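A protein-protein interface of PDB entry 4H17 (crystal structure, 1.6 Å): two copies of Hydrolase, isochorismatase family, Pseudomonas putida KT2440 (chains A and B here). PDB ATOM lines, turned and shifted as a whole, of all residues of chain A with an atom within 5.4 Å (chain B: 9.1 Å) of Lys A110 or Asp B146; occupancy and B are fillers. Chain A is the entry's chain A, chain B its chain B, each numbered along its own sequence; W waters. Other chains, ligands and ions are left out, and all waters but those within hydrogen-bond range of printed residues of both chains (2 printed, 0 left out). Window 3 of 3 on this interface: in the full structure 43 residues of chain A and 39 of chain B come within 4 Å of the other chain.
Met A105 touches Lys B145 (CE to O, 3.7 Å).
Asp B146 touches Met A105 (OD1 to CB, 3.6 Å).
CD of Pro A106 touches CE of Lys B145 (3.9 Å).
Pro A106 touches Asn B186 (CG to ND2, 3.8 Å).
CE1 of Phe B187 touches CG of Pro A106 (3.8 Å).
Asn A107 touches Arg B143.
Lys A110 touches Asp B146 (CE to O, 3.5 Å).
Water W2 lies within hydrogen-bond range of OD1 of Asp B146 and N of Asn A107.
Water W1 bridges NH2 of Arg B143 (3.2 Å) and NZ of Lys A110 (3.2 Å).
Of the printed residues of chain B, Lys A110 touches Asp B146 (3.5 Å).
Printed residues of chain A within 4 Å of Asp B146: Met A105, Asn A107 and Lys A110.
Asn A107 touches just these residues of chain B: Arg B143 (3.7 Å) and Asp B146 (2.8 Å).
No residue of chain B comes within 4 Å of Asn A111.
Of the printed residues of chain A, Arg B143 touches Asn A107 (3.7 Å).
Printed residues of chain A within 4 Å of Asn B186: Pro A106 (3.8 Å).
Of the printed residues of chain B, Pro A106 touches Lys B145 (3.9 Å), Asn B186 (3.8 Å) and Phe B187 (3.8 Å).
Printed residues of chain B within 4 Å of Met A105: Lys B145 and Asp B146.
Tyr B149 touches none of the printed residues of chain A.
Asn B107 touches none of the printed residues of chain A.
The nearest printed residue of chain A that does not touch Asp B146 is Pro A106 (5.3 Å).
The nearest printed residue of chain A that does not touch Arg B143 is Lys A110 (4.8 Å).
Of the 10 printed residues of chain A, 4 touch a printed residue of chain B.
Along chain A the printed residues that touch a printed residue of chain B span positions 105 to 110.
Of the 19 printed residues of chain B, 5 touch a printed residue of chain A.
Hydrophobic or aromatic side chains of chain B within 4 Å of the printed part of chain A: Phe B187.
Among the printed residues, no Asp or Glu carboxylate lies within 4 Å of a Lys or Arg side-chain nitrogen of the other chain.
The backbone NH (N) of Phe A109 sits at hydrogen-bond distance from the side-chain amide oxygen (OD1) of Asn A107, 2.9 Å away.
NZ of Lys B145 lies within hydrogen-bond range of O of Asn B186 (2.7 Å).
The side-chain amino group (NZ) of Lys A103 lies within hydrogen-bond range of the backbone carbonyl oxygen (O) of Met A105, 2.7 Å away.
NH2 of Arg B143 is in hydrogen-bond range of OH of Tyr B147 (3.3 Å).
The guanidinium group of Arg B143 lies within salt-bridge range of the side-chain carboxylate of Asp B146 (2.8 Å).
OD2 of Asp B146 lies within hydrogen-bond range of ND2 of Asn A107, 2.8 Å away.
2 positions are printed for both chains.
Of the 8 pairs that touch across the chains among the printed residues, none has its exchanged pair printed and touching as well.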
ATOM      1  N   LYS A 103       9.010  10.414  17.045  1.00  0.00           N
ATOM      2  CA  LYS A 103       8.007   9.381  16.789  1.00  0.00           C
ATOM      3  C   LYS A 103       7.490   8.701  18.075  1.00  0.00           C
ATOM      4  O   LYS A 103       8.237   8.579  19.091  1.00  0.00           O
ATOM      5  CB  LYS A 103       8.606   8.337  15.851  1.00  0.00           C
ATOM      6  CG  LYS A 103       9.661   7.475  16.522  1.00  0.00           C
ATOM      7  CD  LYS A 103      10.152   6.360  15.612  1.00  0.00           C
ATOM      8  CE  LYS A 103      11.028   5.397  16.375  1.00  0.00           C
ATOM      9  NZ  LYS A 103      10.355   4.591  17.407  1.00  0.00           N
ATOM     10  N   ARG A 104       6.256   8.197  18.015  1.00  0.00           N
ATOM     11  CA  ARG A 104       5.669   7.440  19.133  1.00  0.00           C
ATOM     12  C   ARG A 104       5.802   5.920  19.004  1.00  0.00           C
ATOM     13  O   ARG A 104       5.956   5.219  20.017  1.00  0.00           O
ATOM     14  CB  ARG A 104       4.192   7.786  19.352  1.00  0.00           C
ATOM     15  CG  ARG A 104       3.647   7.101  20.610  1.00  0.00           C
ATOM     16  CD  ARG A 104       4.420   7.437  21.894  1.00  0.00           C
ATOM     17  NE  ARG A 104       4.169   8.824  22.196  1.00  0.00           N
ATOM     18  CZ  ARG A 104       4.762   9.569  23.129  1.00  0.00           C
ATOM     19  NH1 ARG A 104       5.738   9.105  23.890  1.00  0.00           N
ATOM     20  NH2 ARG A 104       4.371  10.825  23.264  1.00  0.00           N
ATOM     21  N   MET A 105       5.762   5.420  17.768  1.00  0.00           N
ATOM     22  CA  MET A 105       5.701   3.993  17.551  1.00  0.00           C
ATOM     23  C   MET A 105       7.010   3.463  17.080  1.00  0.00           C
ATOM     24  O   MET A 105       7.821   4.215  16.492  1.00  0.00           O
ATOM     25  CB  MET A 105       4.657   3.637  16.475  1.00  0.00           C
ATOM     26  CG  MET A 105       3.323   4.296  16.684  1.00  0.00           C
ATOM     27  SD  MET A 105       2.540   3.921  18.416  1.00  0.00           S
ATOM     28  CE  MET A 105       2.504   2.023  18.238  1.00  0.00           C
ATOM     29  N   PRO A 106       7.240   2.140  17.205  1.00  0.00           N
ATOM     30  CA  PRO A 106       8.423   1.531  16.550  1.00  0.00           C
ATOM     31  C   PRO A 106       8.489   1.819  15.045  1.00  0.00           C
ATOM     32  O   PRO A 106       9.551   2.077  14.530  1.00  0.00           O
ATOM     33  CB  PRO A 106       8.274   0.032  16.853  1.00  0.00           C
ATOM     34  CG  PRO A 106       7.523  -0.004  18.150  1.00  0.00           C
ATOM     35  CD  PRO A 106       6.547   1.158  18.074  1.00  0.00           C
ATOM     36  N   ASN A 107       7.336   1.834  14.382  1.00  0.00           N
ATOM     37  CA  ASN A 107       7.195   2.274  13.014  1.00  0.00           C
ATOM     38  C   ASN A 107       7.385   3.797  12.919  1.00  0.00           C
ATOM     39  O   ASN A 107       6.506   4.570  13.279  1.00  0.00           O
ATOM     40  CB  ASN A 107       5.799   1.890  12.517  1.00  0.00           C
ATOM     41  CG  ASN A 107       5.466   2.472  11.165  1.00  0.00           C
ATOM     42  OD1 ASN A 107       6.358   3.005  10.458  1.00  0.00           O
ATOM     43  ND2 ASN A 107       4.209   2.432  10.812  1.00  0.00           N
ATOM     44  N   ALA A 108       8.527   4.210  12.348  1.00  0.00           N
ATOM     45  CA  ALA A 108       8.850   5.626  12.272  1.00  0.00           C
ATOM     46  C   ALA A 108       8.009   6.435  11.280  1.00  0.00           C
ATOM     47  O   ALA A 108       8.094   7.669  11.275  1.00  0.00           O
ATOM     48  CB  ALA A 108      10.337   5.857  11.997  1.00  0.00           C
ATOM     49  N   PHE A 109       7.206   5.752  10.449  1.00  0.00           N
ATOM     50  CA  PHE A 109       6.227   6.448   9.578  1.00  0.00           C
ATOM     51  C   PHE A 109       4.983   6.946  10.297  1.00  0.00           C
ATOM     52  O   PHE A 109       4.346   7.913   9.848  1.00  0.00           O
ATOM     53  CB  PHE A 109       5.815   5.535   8.429  1.00  0.00           C
ATOM     54  CG  PHE A 109       6.936   5.237   7.458  1.00  0.00           C
ATOM     55  CD1 PHE A 109       7.757   4.138   7.665  1.00  0.00           C
ATOM     56  CD2 PHE A 109       7.157   6.033   6.340  1.00  0.00           C
ATOM     57  CE1 PHE A 109       8.749   3.834   6.791  1.00  0.00           C
ATOM     58  CE2 PHE A 109       8.211   5.759   5.480  1.00  0.00           C
ATOM     59  CZ  PHE A 109       8.976   4.637   5.692  1.00  0.00           C
ATOM     60  N   LYS A 110       4.576   6.248  11.363  1.00  0.00           N
ATOM     61  CA  LYS A 110       3.265   6.477  11.967  1.00  0.00           C
ATOM     62  C   LYS A 110       3.182   7.843  12.619  1.00  0.00           C
ATOM     63  O   LYS A 110       3.893   8.131  13.582  1.00  0.00           O
ATOM     64  CB  LYS A 110       2.933   5.365  12.964  1.00  0.00           C
ATOM     65  CG  LYS A 110       1.629   5.518  13.740  1.00  0.00           C
ATOM     66  CD  LYS A 110       0.370   5.551  12.875  1.00  0.00           C
ATOM     67  CE  LYS A 110      -0.889   5.212  13.686  1.00  0.00           C
ATOM     68  NZ  LYS A 110      -2.110   5.049  12.828  1.00  0.00           N
ATOM     69  N   ASN A 111       2.309   8.679  12.058  1.00  0.00           N
ATOM     70  CA  ASN A 111       2.105  10.066  12.513  1.00  0.00           C
ATOM     71  C   ASN A 111       3.341  10.977  12.504  1.00  0.00           C
ATOM     72  O   ASN A 111       3.429  11.916  13.297  1.00  0.00           O
ATOM     73  CB  ASN A 111       1.444  10.089  13.901  1.00  0.00           C
ATOM     74  CG  ASN A 111       0.117   9.348  13.942  1.00  0.00           C
ATOM     75  OD1 ASN A 111      -0.686   9.391  12.997  1.00  0.00           O
ATOM     76  ND2 ASN A 111      -0.142   8.682  15.062  1.00  0.00           N
ATOM     77  N   THR A 112       4.256  10.755  11.552  1.00  0.00           N
ATOM     78  CA  THR A 112       5.479  11.594  11.447  1.00  0.00           C
ATOM     79  C   THR A 112       5.667  12.322  10.095  1.00  0.00           C
ATOM     80  O   THR A 112       6.562  13.146   9.938  1.00  0.00           O
ATOM     81  CB  THR A 112       6.746  10.760  11.653  1.00  0.00           C
ATOM     82  OG1 THR A 112       6.836   9.820  10.566  1.00  0.00           O
ATOM     83  CG2 THR A 112       6.757  10.058  13.005  1.00  0.00           C
ATOM     84  N   ASN B 107       2.769  -7.875   5.355  1.00  0.00           N
ATOM     85  CA  ASN B 107       1.793  -7.127   6.160  1.00  0.00           C
ATOM     86  C   ASN B 107       0.400  -7.469   5.676  1.00  0.00           C
ATOM     87  O   ASN B 107      -0.036  -7.045   4.581  1.00  0.00           O
ATOM     88  CB  ASN B 107       2.067  -5.640   6.045  1.00  0.00           C
ATOM     89  CG  ASN B 107       0.966  -4.794   6.626  1.00  0.00           C
ATOM     90  OD1 ASN B 107       0.047  -5.284   7.297  1.00  0.00           O
ATOM     91  ND2 ASN B 107       1.023  -3.514   6.334  1.00  0.00           N
ATOM     92  N   PHE B 109      -2.438  -6.402   6.492  1.00  0.00           N
ATOM     93  CA  PHE B 109      -3.340  -5.263   6.345  1.00  0.00           C
ATOM     94  C   PHE B 109      -3.250  -4.561   4.968  1.00  0.00           C
ATOM     95  O   PHE B 109      -4.190  -3.902   4.503  1.00  0.00           O
ATOM     96  CB  PHE B 109      -3.050  -4.235   7.439  1.00  0.00           C
ATOM     97  CG  PHE B 109      -3.355  -4.705   8.832  1.00  0.00           C
ATOM     98  CD1 PHE B 109      -2.340  -5.261   9.618  1.00  0.00           C
ATOM     99  CD2 PHE B 109      -4.584  -4.592   9.390  1.00  0.00           C
ATOM    100  CE1 PHE B 109      -2.576  -5.654  10.905  1.00  0.00           C
ATOM    101  CE2 PHE B 109      -4.842  -4.988  10.683  1.00  0.00           C
ATOM    102  CZ  PHE B 109      -3.835  -5.522  11.465  1.00  0.00           C
ATOM    103  N   HIS B 115      -8.068  -4.402   8.368  1.00  0.00           N
ATOM    104  CA  HIS B 115      -8.377  -3.385   9.375  1.00  0.00           C
ATOM    105  C   HIS B 115      -9.869  -3.127   9.536  1.00  0.00           C
ATOM    106  O   HIS B 115     -10.394  -3.194  10.666  1.00  0.00           O
ATOM    107  CB  HIS B 115      -7.657  -2.086   9.109  1.00  0.00           C
ATOM    108  CG  HIS B 115      -7.740  -1.118  10.248  1.00  0.00           C
ATOM    109  ND1 HIS B 115      -7.796   0.247  10.075  1.00  0.00           N
ATOM    110  CD2 HIS B 115      -7.763  -1.330  11.583  1.00  0.00           C
ATOM    111  CE1 HIS B 115      -7.869   0.830  11.260  1.00  0.00           C
ATOM    112  NE2 HIS B 115      -7.832  -0.103  12.189  1.00  0.00           N
ATOM    113  N   GLN B 119     -12.093  -3.938  12.898  1.00  0.00           N
ATOM    114  CA  GLN B 119     -12.854  -2.876  13.517  1.00  0.00           C
ATOM    115  C   GLN B 119     -14.319  -3.269  13.621  1.00  0.00           C
ATOM    116  O   GLN B 119     -14.949  -3.020  14.658  1.00  0.00           O
ATOM    117  CB  GLN B 119     -12.653  -1.562  12.783  1.00  0.00           C
ATOM    118  CG  GLN B 119     -11.243  -1.003  12.924  1.00  0.00           C
ATOM    119  CD  GLN B 119     -10.879  -0.654  14.359  1.00  0.00           C
ATOM    120  OE1 GLN B 119     -10.045  -1.316  14.983  1.00  0.00           O
ATOM    121  NE2 GLN B 119     -11.522   0.365  14.896  1.00  0.00           N
ATOM    122  N   THR B 139       5.549  -9.274  10.702  1.00  0.00           N
ATOM    123  CA  THR B 139       5.145  -8.012  10.061  1.00  0.00           C
ATOM    124  C   THR B 139       3.733  -7.608  10.425  1.00  0.00           C
ATOM    125  O   THR B 139       3.471  -6.419  10.771  1.00  0.00           O
ATOM    126  CB  THR B 139       5.278  -8.116   8.546  1.00  0.00           C
ATOM    127  OG1 THR B 139       6.625  -8.496   8.216  1.00  0.00           O
ATOM    128  CG2 THR B 139       4.941  -6.820   7.920  1.00  0.00           C
ATOM    129  N   THR B 140       2.808  -8.566  10.342  1.00  0.00           N
ATOM    130  CA  THR B 140       1.404  -8.287  10.630  1.00  0.00           C
ATOM    131  C   THR B 140       1.171  -7.884  12.110  1.00  0.00           C
ATOM    132  O   THR B 140       0.456  -6.923  12.384  1.00  0.00           O
ATOM    133  CB  THR B 140       0.527  -9.466  10.220  1.00  0.00           C
ATOM    134  OG1 THR B 140       0.639  -9.643   8.797  1.00  0.00           O
ATOM    135  CG2 THR B 140      -0.921  -9.233  10.558  1.00  0.00           C
ATOM    136  N   VAL B 141       1.837  -8.569  13.026  1.00  0.00           N
ATOM    137  CA  VAL B 141       1.758  -8.297  14.455  1.00  0.00           C
ATOM    138  C   VAL B 141       2.350  -6.896  14.728  1.00  0.00           C
ATOM    139  O   VAL B 141       1.743  -6.087  15.448  1.00  0.00           O
ATOM    140  CB  VAL B 141       2.483  -9.397  15.288  1.00  0.00           C
ATOM    141  CG1 VAL B 141       2.654  -8.997  16.762  1.00  0.00           C
ATOM    142  CG2 VAL B 141       1.742 -10.734  15.226  1.00  0.00           C
ATOM    143  N   ARG B 142       3.475  -6.564  14.097  1.00  0.00           N
ATOM    144  CA  ARG B 142       4.042  -5.213  14.233  1.00  0.00           C
ATOM    145  C   ARG B 142       3.072  -4.129  13.741  1.00  0.00           C
ATOM    146  O   ARG B 142       2.901  -3.121  14.389  1.00  0.00           O
ATOM    147  CB  ARG B 142       5.409  -5.092  13.568  1.00  0.00           C
ATOM    148  CG  ARG B 142       6.472  -6.020  14.135  1.00  0.00           C
ATOM    149  CD  ARG B 142       7.670  -6.081  13.213  1.00  0.00           C
ATOM    150  NE  ARG B 142       8.705  -6.996  13.703  1.00  0.00           N
ATOM    151  CZ  ARG B 142       9.755  -6.639  14.426  1.00  0.00           C
ATOM    152  NH1 ARG B 142       9.904  -5.373  14.807  1.00  0.00           N
ATOM    153  NH2 ARG B 142      10.614  -7.561  14.819  1.00  0.00           N
ATOM    154  N   ARG B 143       2.439  -4.370  12.596  1.00  0.00           N
ATOM    155  CA  ARG B 143       1.466  -3.389  12.039  1.00  0.00           C
ATOM    156  C   ARG B 143       0.241  -3.211  12.961  1.00  0.00           C
ATOM    157  O   ARG B 143      -0.230  -2.102  13.166  1.00  0.00           O
ATOM    158  CB  ARG B 143       1.032  -3.773  10.619  1.00  0.00           C
ATOM    159  CG  ARG B 143       0.161  -2.736   9.931  1.00  0.00           C
ATOM    160  CD  ARG B 143       0.769  -1.340   9.902  1.00  0.00           C
ATOM    161  NE  ARG B 143      -0.108  -0.394   9.208  1.00  0.00           N
ATOM    162  CZ  ARG B 143      -0.069   0.928   9.365  1.00  0.00           C
ATOM    163  NH1 ARG B 143       0.714   1.458  10.305  1.00  0.00           N
ATOM    164  NH2 ARG B 143      -0.874   1.710   8.657  1.00  0.00           N
ATOM    165  N   ALA B 144      -0.231  -4.307  13.552  1.00  0.00           N
ATOM    166  CA  ALA B 144      -1.355  -4.307  14.464  1.00  0.00           C
ATOM    167  C   ALA B 144      -1.095  -3.412  15.668  1.00  0.00           C
ATOM    168  O   ALA B 144      -2.020  -2.798  16.164  1.00  0.00           O
ATOM    169  CB  ALA B 144      -1.693  -5.715  14.908  1.00  0.00           C
ATOM    170  N   LYS B 145       0.168  -3.318  16.105  1.00  0.00           N
ATOM    171  CA  LYS B 145       0.526  -2.360  17.177  1.00  0.00           C
ATOM    172  C   LYS B 145       0.125  -0.908  16.845  1.00  0.00           C
ATOM    173  O   LYS B 145      -0.403  -0.208  17.695  1.00  0.00           O
ATOM    174  CB  LYS B 145       2.003  -2.471  17.520  1.00  0.00           C
ATOM    175  CG  LYS B 145       2.409  -1.652  18.749  1.00  0.00           C
ATOM    176  CD  LYS B 145       3.902  -1.802  18.953  1.00  0.00           C
ATOM    177  CE  LYS B 145       4.378  -1.177  20.251  1.00  0.00           C
ATOM    178  NZ  LYS B 145       4.138  -2.002  21.456  1.00  0.00           N
ATOM    179  N   ASP B 146       0.363  -0.505  15.603  1.00  0.00           N
ATOM    180  CA  ASP B 146      -0.013   0.820  15.079  1.00  0.00           C
ATOM    181  C   ASP B 146      -1.465   1.172  15.219  1.00  0.00           C
ATOM    182  O   ASP B 146      -1.822   2.344  15.401  1.00  0.00           O
ATOM    183  CB  ASP B 146       0.445   0.977  13.627  1.00  0.00           C
ATOM    184  CG  ASP B 146       1.974   1.044  13.499  1.00  0.00           C
ATOM    185  OD1 ASP B 146       2.685   1.344  14.507  1.00  0.00           O
ATOM    186  OD2 ASP B 146       2.489   0.796  12.369  1.00  0.00           O
ATOM    187  N   TYR B 147      -2.325   0.161  15.122  1.00  0.00           N
ATOM    188  CA  TYR B 147      -3.759   0.347  15.220  1.00  0.00           C
ATOM    189  C   TYR B 147      -4.264   0.200  16.650  1.00  0.00           C
ATOM    190  O   TYR B 147      -5.468   0.260  16.913  1.00  0.00           O
ATOM    191  CB  TYR B 147      -4.464  -0.656  14.319  1.00  0.00           C
ATOM    192  CG  TYR B 147      -4.290  -0.399  12.837  1.00  0.00           C
ATOM    193  CD1 TYR B 147      -4.679   0.821  12.274  1.00  0.00           C
ATOM    194  CD2 TYR B 147      -3.749  -1.352  11.982  1.00  0.00           C
ATOM    195  CE1 TYR B 147      -4.534   1.082  10.915  1.00  0.00           C
ATOM    196  CE2 TYR B 147      -3.608  -1.100  10.621  1.00  0.00           C
ATOM    197  CZ  TYR B 147      -3.992   0.118  10.090  1.00  0.00           C
ATOM    198  OH  TYR B 147      -3.867   0.409   8.725  1.00  0.00           O
ATOM    199  N   GLY B 148      -3.359  -0.079  17.581  1.00  0.00           N
ATOM    200  CA  GLY B 148      -3.743  -0.257  18.955  1.00  0.00           C
ATOM    201  C   GLY B 148      -4.322  -1.609  19.339  1.00  0.00           C
ATOM    202  O   GLY B 148      -4.876  -1.765  20.434  1.00  0.00           O
ATOM    203  N   TYR B 149      -4.131  -2.620  18.499  1.00  0.00           N
ATOM    204  CA  TYR B 149      -4.534  -3.979  18.852  1.00  0.00           C
ATOM    205  C   TYR B 149      -3.599  -4.599  19.857  1.00  0.00           C
ATOM    206  O   TYR B 149      -2.412  -4.261  19.940  1.00  0.00           O
ATOM    207  CB  TYR B 149      -4.644  -4.938  17.628  1.00  0.00           C
ATOM    208  CG  TYR B 149      -5.753  -4.513  16.698  1.00  0.00           C
ATOM    209  CD1 TYR B 149      -7.091  -4.763  17.017  1.00  0.00           C
ATOM    210  CD2 TYR B 149      -5.477  -3.846  15.514  1.00  0.00           C
ATOM    211  CE1 TYR B 149      -8.110  -4.336  16.179  1.00  0.00           C
ATOM    212  CE2 TYR B 149      -6.497  -3.395  14.680  1.00  0.00           C
ATOM    213  CZ  TYR B 149      -7.803  -3.629  15.021  1.00  0.00           C
ATOM    214  OH  TYR B 149      -8.795  -3.169  14.164  1.00  0.00           O
ATOM    215  N   ARG B 150      -4.164  -5.496  20.653  1.00  0.00           N
ATOM    216  CA  ARG B 150      -3.410  -6.311  21.602  1.00  0.00           C
ATOM    217  C   ARG B 150      -3.272  -7.717  21.038  1.00  0.00           C
ATOM    218  O   ARG B 150      -4.276  -8.397  20.874  1.00  0.00           O
ATOM    219  CB  ARG B 150      -4.191  -6.394  22.909  1.00  0.00           C
ATOM    220  CG  ARG B 150      -4.227  -5.110  23.722  1.00  0.00           C
ATOM    221  CD  ARG B 150      -4.820  -5.391  25.094  1.00  0.00           C
ATOM    222  NE  ARG B 150      -6.238  -5.763  25.047  1.00  0.00           N
ATOM    223  CZ  ARG B 150      -7.250  -4.885  25.035  1.00  0.00           C
ATOM    224  NH1 ARG B 150      -7.026  -3.575  25.075  1.00  0.00           N
ATOM    225  NH2 ARG B 150      -8.508  -5.322  24.995  1.00  0.00           N
ATOM    226  N   CYS B 151      -2.047  -8.148  20.738  1.00  0.00           N
ATOM    227  CA  CYS B 151      -1.775  -9.395  20.080  1.00  0.00           C
ATOM    228  C   CYS B 151      -1.224 -10.404  21.052  1.00  0.00           C
ATOM    229  O   CYS B 151      -0.347 -10.080  21.874  1.00  0.00           O
ATOM    230  CB  CYS B 151      -0.726  -9.207  18.948  1.00  0.00           C
ATOM    231  SG  CYS B 151      -1.394  -8.233  17.580  1.00  0.00           S
ATOM    232  N   ASN B 186       8.168  -6.283  22.797  1.00  0.00           N
ATOM    233  CA  ASN B 186       7.504  -5.071  22.407  1.00  0.00           C
ATOM    234  C   ASN B 186       6.323  -5.153  21.441  1.00  0.00           C
ATOM    235  O   ASN B 186       5.799  -4.118  21.011  1.00  0.00           O
ATOM    236  CB  ASN B 186       8.555  -4.120  21.862  1.00  0.00           C
ATOM    237  CG  ASN B 186       8.212  -2.690  22.089  1.00  0.00           C
ATOM    238  OD1 ASN B 186       7.514  -2.344  23.047  1.00  0.00           O
ATOM    239  ND2 ASN B 186       8.697  -1.846  21.229  1.00  0.00           N
ATOM    240  N   PHE B 187       5.898  -6.360  21.063  1.00  0.00           N
ATOM    241  CA  PHE B 187       4.874  -6.497  20.013  1.00  0.00           C
ATOM    242  C   PHE B 187       3.707  -7.427  20.291  1.00  0.00           C
ATOM    243  O   PHE B 187       2.657  -7.274  19.668  1.00  0.00           O
ATOM    244  CB  PHE B 187       5.570  -6.880  18.721  1.00  0.00           C
ATOM    245  CG  PHE B 187       6.580  -5.850  18.288  1.00  0.00           C
ATOM    246  CD1 PHE B 187       6.166  -4.672  17.698  1.00  0.00           C
ATOM    247  CD2 PHE B 187       7.920  -6.030  18.549  1.00  0.00           C
ATOM    248  CE1 PHE B 187       7.052  -3.718  17.344  1.00  0.00           C
ATOM    249  CE2 PHE B 187       8.849  -5.071  18.200  1.00  0.00           C
ATOM    250  CZ  PHE B 187       8.415  -3.924  17.580  1.00  0.00           C
HETATM  251  O   HOH W   1      -1.589   4.607   9.667  1.00  0.00           O
HETATM  252  O   HOH W   2       4.776   0.495  15.443  1.00  0.00           O
